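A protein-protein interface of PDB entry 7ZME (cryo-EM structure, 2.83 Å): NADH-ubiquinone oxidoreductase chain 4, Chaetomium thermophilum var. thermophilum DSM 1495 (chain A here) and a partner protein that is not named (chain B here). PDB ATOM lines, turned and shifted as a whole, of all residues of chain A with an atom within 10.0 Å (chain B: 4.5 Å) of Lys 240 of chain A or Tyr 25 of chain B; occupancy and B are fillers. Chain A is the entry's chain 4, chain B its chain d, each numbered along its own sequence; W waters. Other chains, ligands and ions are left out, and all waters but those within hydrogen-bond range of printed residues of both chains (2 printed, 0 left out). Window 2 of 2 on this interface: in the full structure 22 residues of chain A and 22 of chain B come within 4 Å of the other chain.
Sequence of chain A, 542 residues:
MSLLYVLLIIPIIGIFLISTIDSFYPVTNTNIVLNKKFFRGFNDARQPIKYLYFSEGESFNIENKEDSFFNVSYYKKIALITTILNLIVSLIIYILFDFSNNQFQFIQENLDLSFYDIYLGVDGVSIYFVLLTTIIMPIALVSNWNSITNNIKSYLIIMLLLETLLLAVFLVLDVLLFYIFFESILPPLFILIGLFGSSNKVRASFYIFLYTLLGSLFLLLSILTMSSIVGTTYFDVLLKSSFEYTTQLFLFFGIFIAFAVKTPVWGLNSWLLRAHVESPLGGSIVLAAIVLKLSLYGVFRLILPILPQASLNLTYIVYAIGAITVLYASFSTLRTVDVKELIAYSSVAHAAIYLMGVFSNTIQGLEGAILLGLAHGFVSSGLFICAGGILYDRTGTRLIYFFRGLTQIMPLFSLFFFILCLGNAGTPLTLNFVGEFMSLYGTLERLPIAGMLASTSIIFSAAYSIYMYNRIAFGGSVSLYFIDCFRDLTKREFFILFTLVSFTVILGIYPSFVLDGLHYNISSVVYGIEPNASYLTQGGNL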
ATOM      1  N   VAL A 230     -31.489   5.081   4.213  1.00  0.00           N
ATOM      2  CA  VAL A 230     -31.191   5.917   5.411  1.00  0.00           C
ATOM      3  C   VAL A 230     -31.666   7.356   5.216  1.00  0.00           C
ATOM      4  O   VAL A 230     -31.913   8.037   6.223  1.00  0.00           O
ATOM      5  CB  VAL A 230     -29.686   5.816   5.726  1.00  0.00           C
ATOM      6  CG1 VAL A 230     -29.261   6.650   6.925  1.00  0.00           C
ATOM      7  CG2 VAL A 230     -29.262   4.371   5.907  1.00  0.00           C
ATOM      8  N   THR A 232     -29.728   9.650   3.853  1.00  0.00           N
ATOM      9  CA  THR A 232     -28.515  10.446   3.720  1.00  0.00           C
ATOM     10  C   THR A 232     -27.332   9.491   3.692  1.00  0.00           C
ATOM     11  O   THR A 232     -27.479   8.286   3.913  1.00  0.00           O
ATOM     12  CB  THR A 232     -28.377  11.469   4.854  1.00  0.00           C
ATOM     13  OG1 THR A 232     -27.245  12.311   4.608  1.00  0.00           O
ATOM     14  CG2 THR A 232     -28.213  10.780   6.184  1.00  0.00           C
ATOM     15  N   THR A 233     -26.158  10.042   3.385  1.00  0.00           N
ATOM     16  CA  THR A 233     -24.898   9.318   3.504  1.00  0.00           C
ATOM     17  C   THR A 233     -23.883  10.043   4.377  1.00  0.00           C
ATOM     18  O   THR A 233     -22.706   9.670   4.376  1.00  0.00           O
ATOM     19  CB  THR A 233     -24.291   9.033   2.126  1.00  0.00           C
ATOM     20  OG1 THR A 233     -24.022  10.263   1.446  1.00  0.00           O
ATOM     21  CG2 THR A 233     -25.200   8.164   1.294  1.00  0.00           C
ATOM     22  N   TYR A 234     -24.305  11.069   5.113  1.00  0.00           N
ATOM     23  CA  TYR A 234     -23.437  11.693   6.101  1.00  0.00           C
ATOM     24  C   TYR A 234     -22.959  10.642   7.093  1.00  0.00           C
ATOM     25  O   TYR A 234     -23.739   9.806   7.552  1.00  0.00           O
ATOM     26  CB  TYR A 234     -24.185  12.817   6.817  1.00  0.00           C
ATOM     27  CG  TYR A 234     -23.355  13.604   7.807  1.00  0.00           C
ATOM     28  CD1 TYR A 234     -22.351  14.460   7.377  1.00  0.00           C
ATOM     29  CD2 TYR A 234     -23.596  13.510   9.169  1.00  0.00           C
ATOM     30  CE1 TYR A 234     -21.602  15.183   8.278  1.00  0.00           C
ATOM     31  CE2 TYR A 234     -22.853  14.230  10.074  1.00  0.00           C
ATOM     32  CZ  TYR A 234     -21.857  15.064   9.625  1.00  0.00           C
ATOM     33  OH  TYR A 234     -21.113  15.784  10.530  1.00  0.00           O
ATOM     34  N   PHE A 235     -21.664  10.684   7.413  1.00  0.00           N
ATOM     35  CA  PHE A 235     -21.035   9.577   8.129  1.00  0.00           C
ATOM     36  C   PHE A 235     -21.719   9.306   9.461  1.00  0.00           C
ATOM     37  O   PHE A 235     -22.040   8.158   9.779  1.00  0.00           O
ATOM     38  CB  PHE A 235     -19.548   9.858   8.341  1.00  0.00           C
ATOM     39  CG  PHE A 235     -18.697   9.561   7.141  1.00  0.00           C
ATOM     40  CD1 PHE A 235     -19.200   8.824   6.085  1.00  0.00           C
ATOM     41  CD2 PHE A 235     -17.391  10.017   7.071  1.00  0.00           C
ATOM     42  CE1 PHE A 235     -18.421   8.554   4.984  1.00  0.00           C
ATOM     43  CE2 PHE A 235     -16.612   9.750   5.974  1.00  0.00           C
ATOM     44  CZ  PHE A 235     -17.124   9.020   4.929  1.00  0.00           C
ATOM     45  N   ASP A 236     -21.972  10.353  10.250  1.00  0.00           N
ATOM     46  CA  ASP A 236     -22.514  10.147  11.590  1.00  0.00           C
ATOM     47  C   ASP A 236     -23.874   9.467  11.542  1.00  0.00           C
ATOM     48  O   ASP A 236     -24.148   8.557  12.332  1.00  0.00           O
ATOM     49  CB  ASP A 236     -22.606  11.479  12.329  1.00  0.00           C
ATOM     50  CG  ASP A 236     -21.248  12.019  12.725  1.00  0.00           C
ATOM     51  OD1 ASP A 236     -20.263  11.254  12.663  1.00  0.00           O
ATOM     52  OD2 ASP A 236     -21.167  13.207  13.103  1.00  0.00           O
ATOM     53  N   VAL A 237     -24.739   9.893  10.624  1.00  0.00           N
ATOM     54  CA  VAL A 237     -26.054   9.274  10.493  1.00  0.00           C
ATOM     55  C   VAL A 237     -25.929   7.864   9.931  1.00  0.00           C
ATOM     56  O   VAL A 237     -26.537   6.917  10.438  1.00  0.00           O
ATOM     57  CB  VAL A 237     -26.967  10.145   9.615  1.00  0.00           C
ATOM     58  CG1 VAL A 237     -28.359   9.545   9.540  1.00  0.00           C
ATOM     59  CG2 VAL A 237     -26.998  11.576  10.130  1.00  0.00           C
ATOM     60  N   LEU A 238     -25.133   7.705   8.874  1.00  0.00           N
ATOM     61  CA  LEU A 238     -25.086   6.433   8.165  1.00  0.00           C
ATOM     62  C   LEU A 238     -24.361   5.360   8.966  1.00  0.00           C
ATOM     63  O   LEU A 238     -24.617   4.168   8.772  1.00  0.00           O
ATOM     64  CB  LEU A 238     -24.422   6.632   6.803  1.00  0.00           C
ATOM     65  CG  LEU A 238     -24.282   5.434   5.865  1.00  0.00           C
ATOM     66  CD1 LEU A 238     -25.627   5.034   5.293  1.00  0.00           C
ATOM     67  CD2 LEU A 238     -23.297   5.750   4.760  1.00  0.00           C
ATOM     68  N   LEU A 239     -23.468   5.757   9.875  1.00  0.00           N
ATOM     69  CA  LEU A 239     -22.681   4.776  10.612  1.00  0.00           C
ATOM     70  C   LEU A 239     -23.517   4.009  11.625  1.00  0.00           C
ATOM     71  O   LEU A 239     -23.224   2.844  11.908  1.00  0.00           O
ATOM     72  CB  LEU A 239     -21.506   5.456  11.311  1.00  0.00           C
ATOM     73  CG  LEU A 239     -20.289   5.711  10.423  1.00  0.00           C
ATOM     74  CD1 LEU A 239     -19.069   6.036  11.260  1.00  0.00           C
ATOM     75  CD2 LEU A 239     -20.042   4.524   9.532  1.00  0.00           C
ATOM     76  N   LYS A 240     -24.548   4.633  12.186  1.00  0.00           N
ATOM     77  CA  LYS A 240     -25.436   3.956  13.116  1.00  0.00           C
ATOM     78  C   LYS A 240     -26.612   3.288  12.416  1.00  0.00           C
ATOM     79  O   LYS A 240     -27.643   3.038  13.046  1.00  0.00           O
ATOM     80  CB  LYS A 240     -25.925   4.930  14.190  1.00  0.00           C
ATOM     81  CG  LYS A 240     -26.779   6.073  13.690  1.00  0.00           C
ATOM     82  CD  LYS A 240     -27.146   6.989  14.842  1.00  0.00           C
ATOM     83  CE  LYS A 240     -28.024   8.135  14.390  1.00  0.00           C
ATOM     84  NZ  LYS A 240     -27.289   9.061  13.499  1.00  0.00           N
ATOM     85  N   SER A 241     -26.471   2.986  11.132  1.00  0.00           N
ATOM     86  CA  SER A 241     -27.458   2.225  10.385  1.00  0.00           C
ATOM     87  C   SER A 241     -27.039   0.764  10.342  1.00  0.00           C
ATOM     88  O   SER A 241     -25.860   0.453  10.152  1.00  0.00           O
ATOM     89  CB  SER A 241     -27.610   2.767   8.965  1.00  0.00           C
ATOM     90  OG  SER A 241     -27.999   4.129   8.976  1.00  0.00           O
ATOM     91  N   SER A 242     -28.005  -0.126  10.524  1.00  0.00           N
ATOM     92  CA  SER A 242     -27.768  -1.566  10.495  1.00  0.00           C
ATOM     93  C   SER A 242     -28.635  -2.152   9.386  1.00  0.00           C
ATOM     94  O   SER A 242     -29.820  -2.428   9.591  1.00  0.00           O
ATOM     95  CB  SER A 242     -28.073  -2.202  11.845  1.00  0.00           C
ATOM     96  OG  SER A 242     -27.871  -3.602  11.799  1.00  0.00           O
ATOM     97  N   PHE A 243     -28.040  -2.340   8.214  1.00  0.00           N
ATOM     98  CA  PHE A 243     -28.781  -2.813   7.060  1.00  0.00           C
ATOM     99  C   PHE A 243     -29.133  -4.286   7.214  1.00  0.00           C
ATOM    100  O   PHE A 243     -28.505  -5.029   7.970  1.00  0.00           O
ATOM    101  CB  PHE A 243     -27.967  -2.598   5.787  1.00  0.00           C
ATOM    102  CG  PHE A 243     -27.772  -1.158   5.441  1.00  0.00           C
ATOM    103  CD1 PHE A 243     -28.801  -0.421   4.881  1.00  0.00           C
ATOM    104  CD2 PHE A 243     -26.572  -0.530   5.702  1.00  0.00           C
ATOM    105  CE1 PHE A 243     -28.626   0.907   4.571  1.00  0.00           C
ATOM    106  CE2 PHE A 243     -26.393   0.797   5.398  1.00  0.00           C
ATOM    107  CZ  PHE A 243     -27.420   1.516   4.830  1.00  0.00           C
ATOM    108  N   ARG A 301     -14.564   3.273   5.294  1.00  0.00           N
ATOM    109  CA  ARG A 301     -15.758   4.105   5.338  1.00  0.00           C
ATOM    110  C   ARG A 301     -16.987   3.463   4.723  1.00  0.00           C
ATOM    111  O   ARG A 301     -18.100   3.792   5.133  1.00  0.00           O
ATOM    112  CB  ARG A 301     -15.514   5.441   4.618  1.00  0.00           C
ATOM    113  CG  ARG A 301     -14.345   6.240   5.131  1.00  0.00           C
ATOM    114  CD  ARG A 301     -14.650   6.789   6.499  1.00  0.00           C
ATOM    115  NE  ARG A 301     -13.624   7.711   6.953  1.00  0.00           N
ATOM    116  CZ  ARG A 301     -13.377   7.973   8.228  1.00  0.00           C
ATOM    117  NH1 ARG A 301     -14.086   7.380   9.175  1.00  0.00           N
ATOM    118  NH2 ARG A 301     -12.422   8.831   8.552  1.00  0.00           N
ATOM    119  N   PRO A 305     -17.729  -0.459   8.453  1.00  0.00           N
ATOM    120  CA  PRO A 305     -18.650   0.041   9.475  1.00  0.00           C
ATOM    121  C   PRO A 305     -20.145  -0.094   9.162  1.00  0.00           C
ATOM    122  O   PRO A 305     -20.935   0.073  10.063  1.00  0.00           O
ATOM    123  CB  PRO A 305     -18.244   1.517   9.510  1.00  0.00           C
ATOM    124  CG  PRO A 305     -17.914   1.850   8.088  1.00  0.00           C
ATOM    125  CD  PRO A 305     -17.201   0.615   7.600  1.00  0.00           C
ATOM    126  N   ILE A 306     -20.498  -0.432   7.933  1.00  0.00           N
ATOM    127  CA  ILE A 306     -21.890  -0.493   7.505  1.00  0.00           C
ATOM    128  C   ILE A 306     -22.256  -1.794   6.807  1.00  0.00           C
ATOM    129  O   ILE A 306     -23.452  -2.050   6.607  1.00  0.00           O
ATOM    130  CB  ILE A 306     -22.253   0.716   6.617  1.00  0.00           C
ATOM    131  CG1 ILE A 306     -21.408   0.727   5.347  1.00  0.00           C
ATOM    132  CG2 ILE A 306     -22.069   2.010   7.381  1.00  0.00           C
ATOM    133  CD1 ILE A 306     -21.856   1.736   4.335  1.00  0.00           C
ATOM    134  N   LEU A 307     -21.287  -2.667   6.550  1.00  0.00           N
ATOM    135  CA  LEU A 307     -21.589  -3.985   5.927  1.00  0.00           C
ATOM    136  C   LEU A 307     -20.912  -5.054   6.771  1.00  0.00           C
ATOM    137  O   LEU A 307     -20.209  -5.882   6.170  1.00  0.00           O
ATOM    138  CB  LEU A 307     -21.107  -4.045   4.474  1.00  0.00           C
ATOM    139  CG  LEU A 307     -21.632  -2.962   3.530  1.00  0.00           C
ATOM    140  CD1 LEU A 307     -20.972  -3.076   2.167  1.00  0.00           C
ATOM    141  CD2 LEU A 307     -23.142  -3.039   3.393  1.00  0.00           C
ATOM    142  N   PRO A 308     -21.104  -5.124   8.106  1.00  0.00           N
ATOM    143  CA  PRO A 308     -20.292  -6.026   8.922  1.00  0.00           C
ATOM    144  C   PRO A 308     -20.448  -7.515   8.618  1.00  0.00           C
ATOM    145  O   PRO A 308     -19.454  -8.179   8.444  1.00  0.00           O
ATOM    146  CB  PRO A 308     -20.887  -5.765  10.302  1.00  0.00           C
ATOM    147  CG  PRO A 308     -21.478  -4.390  10.225  1.00  0.00           C
ATOM    148  CD  PRO A 308     -22.134  -4.423   8.870  1.00  0.00           C
ATOM    149  N   SER A 524     -12.935   1.188  16.183  1.00  0.00           N
ATOM    150  CA  SER A 524     -14.338   1.366  15.847  1.00  0.00           C
ATOM    151  C   SER A 524     -14.761   0.626  14.585  1.00  0.00           C
ATOM    152  O   SER A 524     -15.939   0.685  14.223  1.00  0.00           O
ATOM    153  CB  SER A 524     -14.648   2.853  15.686  1.00  0.00           C
ATOM    154  OG  SER A 524     -13.782   3.453  14.743  1.00  0.00           O
ATOM    155  N   TYR A 535     -21.734  -6.714  26.989  1.00  0.00           N
ATOM    156  CA  TYR A 535     -23.014  -6.540  27.674  1.00  0.00           C
ATOM    157  C   TYR A 535     -22.835  -6.474  29.188  1.00  0.00           C
ATOM    158  O   TYR A 535     -23.623  -7.036  29.951  1.00  0.00           O
ATOM    159  CB  TYR A 535     -23.990  -7.651  27.288  1.00  0.00           C
ATOM    160  CG  TYR A 535     -24.226  -7.745  25.805  1.00  0.00           C
ATOM    161  CD1 TYR A 535     -24.900  -6.742  25.128  1.00  0.00           C
ATOM    162  CD2 TYR A 535     -23.760  -8.825  25.078  1.00  0.00           C
ATOM    163  CE1 TYR A 535     -25.113  -6.821  23.770  1.00  0.00           C
ATOM    164  CE2 TYR A 535     -23.967  -8.911  23.720  1.00  0.00           C
ATOM    165  CZ  TYR A 535     -24.645  -7.907  23.071  1.00  0.00           C
ATOM    166  OH  TYR A 535     -24.854  -7.989  21.718  1.00  0.00           O
ATOM    167  N   PHE B  20     -24.842  -0.124  25.761  1.00  0.00           N
ATOM    168  CA  PHE B  20     -25.765   0.422  24.776  1.00  0.00           C
ATOM    169  C   PHE B  20     -27.214   0.260  25.217  1.00  0.00           C
ATOM    170  O   PHE B  20     -28.128   0.374  24.397  1.00  0.00           O
ATOM    171  CB  PHE B  20     -25.547  -0.232  23.412  1.00  0.00           C
ATOM    172  CG  PHE B  20     -24.380   0.323  22.659  1.00  0.00           C
ATOM    173  CD1 PHE B  20     -24.435   1.590  22.113  1.00  0.00           C
ATOM    174  CD2 PHE B  20     -23.227  -0.419  22.503  1.00  0.00           C
ATOM    175  CE1 PHE B  20     -23.365   2.107  21.427  1.00  0.00           C
ATOM    176  CE2 PHE B  20     -22.153   0.092  21.818  1.00  0.00           C
ATOM    177  CZ  PHE B  20     -22.222   1.359  21.278  1.00  0.00           C
ATOM    178  N   VAL B  23     -29.994   3.716  25.800  1.00  0.00           N
ATOM    179  CA  VAL B  23     -29.390   4.840  25.097  1.00  0.00           C
ATOM    180  C   VAL B  23     -30.221   5.121  23.854  1.00  0.00           C
ATOM    181  O   VAL B  23     -30.608   4.194  23.131  1.00  0.00           O
ATOM    182  CB  VAL B  23     -27.918   4.568  24.737  1.00  0.00           C
ATOM    183  CG1 VAL B  23     -27.119   4.302  25.987  1.00  0.00           C
ATOM    184  CG2 VAL B  23     -27.786   3.409  23.781  1.00  0.00           C
ATOM    185  N   ASP B  24     -30.536   6.390  23.632  1.00  0.00           N
ATOM    186  CA  ASP B  24     -31.280   6.805  22.450  1.00  0.00           C
ATOM    187  C   ASP B  24     -30.279   7.104  21.341  1.00  0.00           C
ATOM    188  O   ASP B  24     -29.514   8.068  21.433  1.00  0.00           O
ATOM    189  CB  ASP B  24     -32.148   8.021  22.758  1.00  0.00           C
ATOM    190  CG  ASP B  24     -33.258   8.212  21.747  1.00  0.00           C
ATOM    191  OD1 ASP B  24     -33.460   7.308  20.909  1.00  0.00           O
ATOM    192  OD2 ASP B  24     -33.928   9.266  21.789  1.00  0.00           O
ATOM    193  N   TYR B  25     -30.283   6.276  20.294  1.00  0.00           N
ATOM    194  CA  TYR B  25     -29.352   6.482  19.191  1.00  0.00           C
ATOM    195  C   TYR B  25     -29.607   7.799  18.469  1.00  0.00           C
ATOM    196  O   TYR B  25     -28.733   8.271  17.734  1.00  0.00           O
ATOM    197  CB  TYR B  25     -29.421   5.314  18.201  1.00  0.00           C
ATOM    198  CG  TYR B  25     -28.808   4.011  18.688  1.00  0.00           C
ATOM    199  CD1 TYR B  25     -28.532   3.801  20.029  1.00  0.00           C
ATOM    200  CD2 TYR B  25     -28.504   2.993  17.796  1.00  0.00           C
ATOM    201  CE1 TYR B  25     -27.979   2.618  20.467  1.00  0.00           C
ATOM    202  CE2 TYR B  25     -27.949   1.805  18.228  1.00  0.00           C
ATOM    203  CZ  TYR B  25     -27.688   1.624  19.567  1.00  0.00           C
ATOM    204  OH  TYR B  25     -27.131   0.450  20.008  1.00  0.00           O
ATOM    205  N   GLU B  26     -30.759   8.415  18.754  1.00  0.00           N
ATOM    206  CA  GLU B  26     -31.067   9.750  18.181  1.00  0.00           C
ATOM    207  C   GLU B  26     -30.212  10.792  18.906  1.00  0.00           C
ATOM    208  O   GLU B  26     -29.935  11.846  18.302  1.00  0.00           O
ATOM    209  CB  GLU B  26     -32.557  10.061  18.336  1.00  0.00           C
ATOM    210  CG  GLU B  26     -33.382   9.710  17.112  1.00  0.00           C
ATOM    211  CD  GLU B  26     -33.523   8.229  16.805  1.00  0.00           C
ATOM    212  OE1 GLU B  26     -33.332   7.409  17.726  1.00  0.00           O
ATOM    213  OE2 GLU B  26     -33.823   7.900  15.642  1.00  0.00           O
ATOM    214  N   ASP B  27     -29.791  10.500  20.142  1.00  0.00           N
ATOM    215  CA  ASP B  27     -28.869  11.432  20.847  1.00  0.00           C
ATOM    216  C   ASP B  27     -27.463  11.087  20.369  1.00  0.00           C
ATOM    217  O   ASP B  27     -26.932  10.049  20.790  1.00  0.00           O
ATOM    218  CB  ASP B  27     -29.006  11.337  22.368  1.00  0.00           C
ATOM    219  CG  ASP B  27     -28.204  12.385  23.123  1.00  0.00           C
ATOM    220  OD1 ASP B  27     -27.593  13.251  22.464  1.00  0.00           O
ATOM    221  OD2 ASP B  27     -28.201  12.331  24.368  1.00  0.00           O
ATOM    222  N   ASN B  28     -26.903  11.931  19.506  1.00  0.00           N
ATOM    223  CA  ASN B  28     -25.584  11.629  18.902  1.00  0.00           C
ATOM    224  C   ASN B  28     -24.528  11.610  19.993  1.00  0.00           C
ATOM    225  O   ASN B  28     -23.691  10.703  19.965  1.00  0.00           O
ATOM    226  CB  ASN B  28     -25.264  12.637  17.802  1.00  0.00           C
ATOM    227  CG  ASN B  28     -26.455  12.894  16.906  1.00  0.00           C
ATOM    228  OD1 ASN B  28     -26.996  11.968  16.306  1.00  0.00           O
ATOM    229  ND2 ASN B  28     -26.875  14.145  16.812  1.00  0.00           N
ATOM    230  N   LEU B  31     -24.698   8.374  22.084  1.00  0.00           N
ATOM    231  CA  LEU B  31     -24.291   7.161  21.340  1.00  0.00           C
ATOM    232  C   LEU B  31     -22.770   7.149  21.255  1.00  0.00           C
ATOM    233  O   LEU B  31     -22.185   6.099  21.508  1.00  0.00           O
ATOM    234  CB  LEU B  31     -24.910   7.208  19.942  1.00  0.00           C
ATOM    235  CG  LEU B  31     -24.513   6.060  19.018  1.00  0.00           C
ATOM    236  CD1 LEU B  31     -25.021   4.735  19.553  1.00  0.00           C
ATOM    237  CD2 LEU B  31     -25.026   6.295  17.613  1.00  0.00           C
ATOM    238  N   GLU B  93     -22.167  -4.839  19.609  1.00  0.00           N
ATOM    239  CA  GLU B  93     -23.125  -4.549  20.669  1.00  0.00           C
ATOM    240  C   GLU B  93     -24.076  -3.430  20.274  1.00  0.00           C
ATOM    241  O   GLU B  93     -25.235  -3.426  20.702  1.00  0.00           O
ATOM    242  CB  GLU B  93     -22.399  -4.185  21.960  1.00  0.00           C
ATOM    243  CG  GLU B  93     -21.907  -5.375  22.751  1.00  0.00           C
ATOM    244  CD  GLU B  93     -21.439  -4.990  24.134  1.00  0.00           C
ATOM    245  OE1 GLU B  93     -22.243  -4.415  24.893  1.00  0.00           O
ATOM    246  OE2 GLU B  93     -20.263  -5.250  24.459  1.00  0.00           O
ATOM    247  N   GLN B  94     -23.608  -2.472  19.475  1.00  0.00           N
ATOM    248  CA  GLN B  94     -24.467  -1.381  19.043  1.00  0.00           C
ATOM    249  C   GLN B  94     -25.590  -1.852  18.131  1.00  0.00           C
ATOM    250  O   GLN B  94     -26.584  -1.139  17.973  1.00  0.00           O
ATOM    251  CB  GLN B  94     -23.638  -0.313  18.337  1.00  0.00           C
ATOM    252  CG  GLN B  94     -24.334   1.025  18.210  1.00  0.00           C
ATOM    253  CD  GLN B  94     -23.557   2.003  17.372  1.00  0.00           C
ATOM    254  OE1 GLN B  94     -22.438   2.376  17.714  1.00  0.00           O
ATOM    255  NE2 GLN B  94     -24.145   2.425  16.263  1.00  0.00           N
HETATM  256  O   HOH W   1     -26.646   0.425  14.843  1.00  0.00           O
HETATM  257  O   HOH W   2     -21.815   3.999  14.766  1.00  0.00           O
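Hydrophobic or aromatic side chains of chain A within 4 Å of the printed part of chain B: Tyr 535.
Printed residues of chain B that touch a printed residue of chain A: Tyr 25, Leu 31, Glu 93 and Gln 94.
Hydrophobic or aromatic side chains of chain B that line the printed part of chain A: Leu 31.
Water W2 bridges the side-chain amide nitrogen of Gln 94 of chain B (3.2 Å) and the backbone carbonyl oxygen of Leu 239 of chain A (3.4 Å).
Water W1 bridges O of Lys 240 of chain A (3.3 Å) and O of Gln 94 of chain B (3.5 Å).
N of Tyr 535 of chain A is in hydrogen-bond range of OE1 of Glu 93 of chain B (3.2 Å).
Asp 236 of chain A touches none of the printed residues of chain B.
Leu 239 of chain A touches none of the printed residues of chain B.
Of chain B, only Tyr 25 (3.4 Å), Leu 31 (3.6 Å) and Gln 94 (3.7 Å) come within 4 Å of Lys 240 of chain A.
Of the printed residues of chain B, Tyr 535 of chain A touches Glu 93.
No residue of chain A comes within 4 Å of Val 23 of chain B.
Of chain A, only Lys 240 (3.4 Å) comes within 4 Å of Tyr 25 of chain B.
No residue of chain A comes within 4 Å of Glu 26 of chain B.
Of the printed residues of chain A, Glu 93 of chain B touches Tyr 535.
Of chain A, only Lys 240 (3.7 Å) comes within 4 Å of Gln 94 of chain B.
The nearest residue of chain A that does not touch Tyr 25 of chain B is Ser 241 of chain A (7.0 Å).
The nearest printed residue of chain A that does not touch Leu 31 of chain B is Asp 236 of chain A (5.8 Å).
Tyr 25 of chain B touches Lys 240 of chain A.
CD of Lys 240 of chain A touches CD2 of Leu 31 of chain B, 3.6 Å away.
Lys 240 of chain A touches Gln 94 of chain B (CB to NE2, 3.7 Å).
OH of Tyr 25 of chain B sits at hydrogen-bond distance from O of Gln 94 of chain B.
The side-chain amino group (NZ) of Lys 240 of chain A is in hydrogen-bond range of the backbone carbonyl oxygen (O) of Asp 236 of chain A (3.4 Å).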
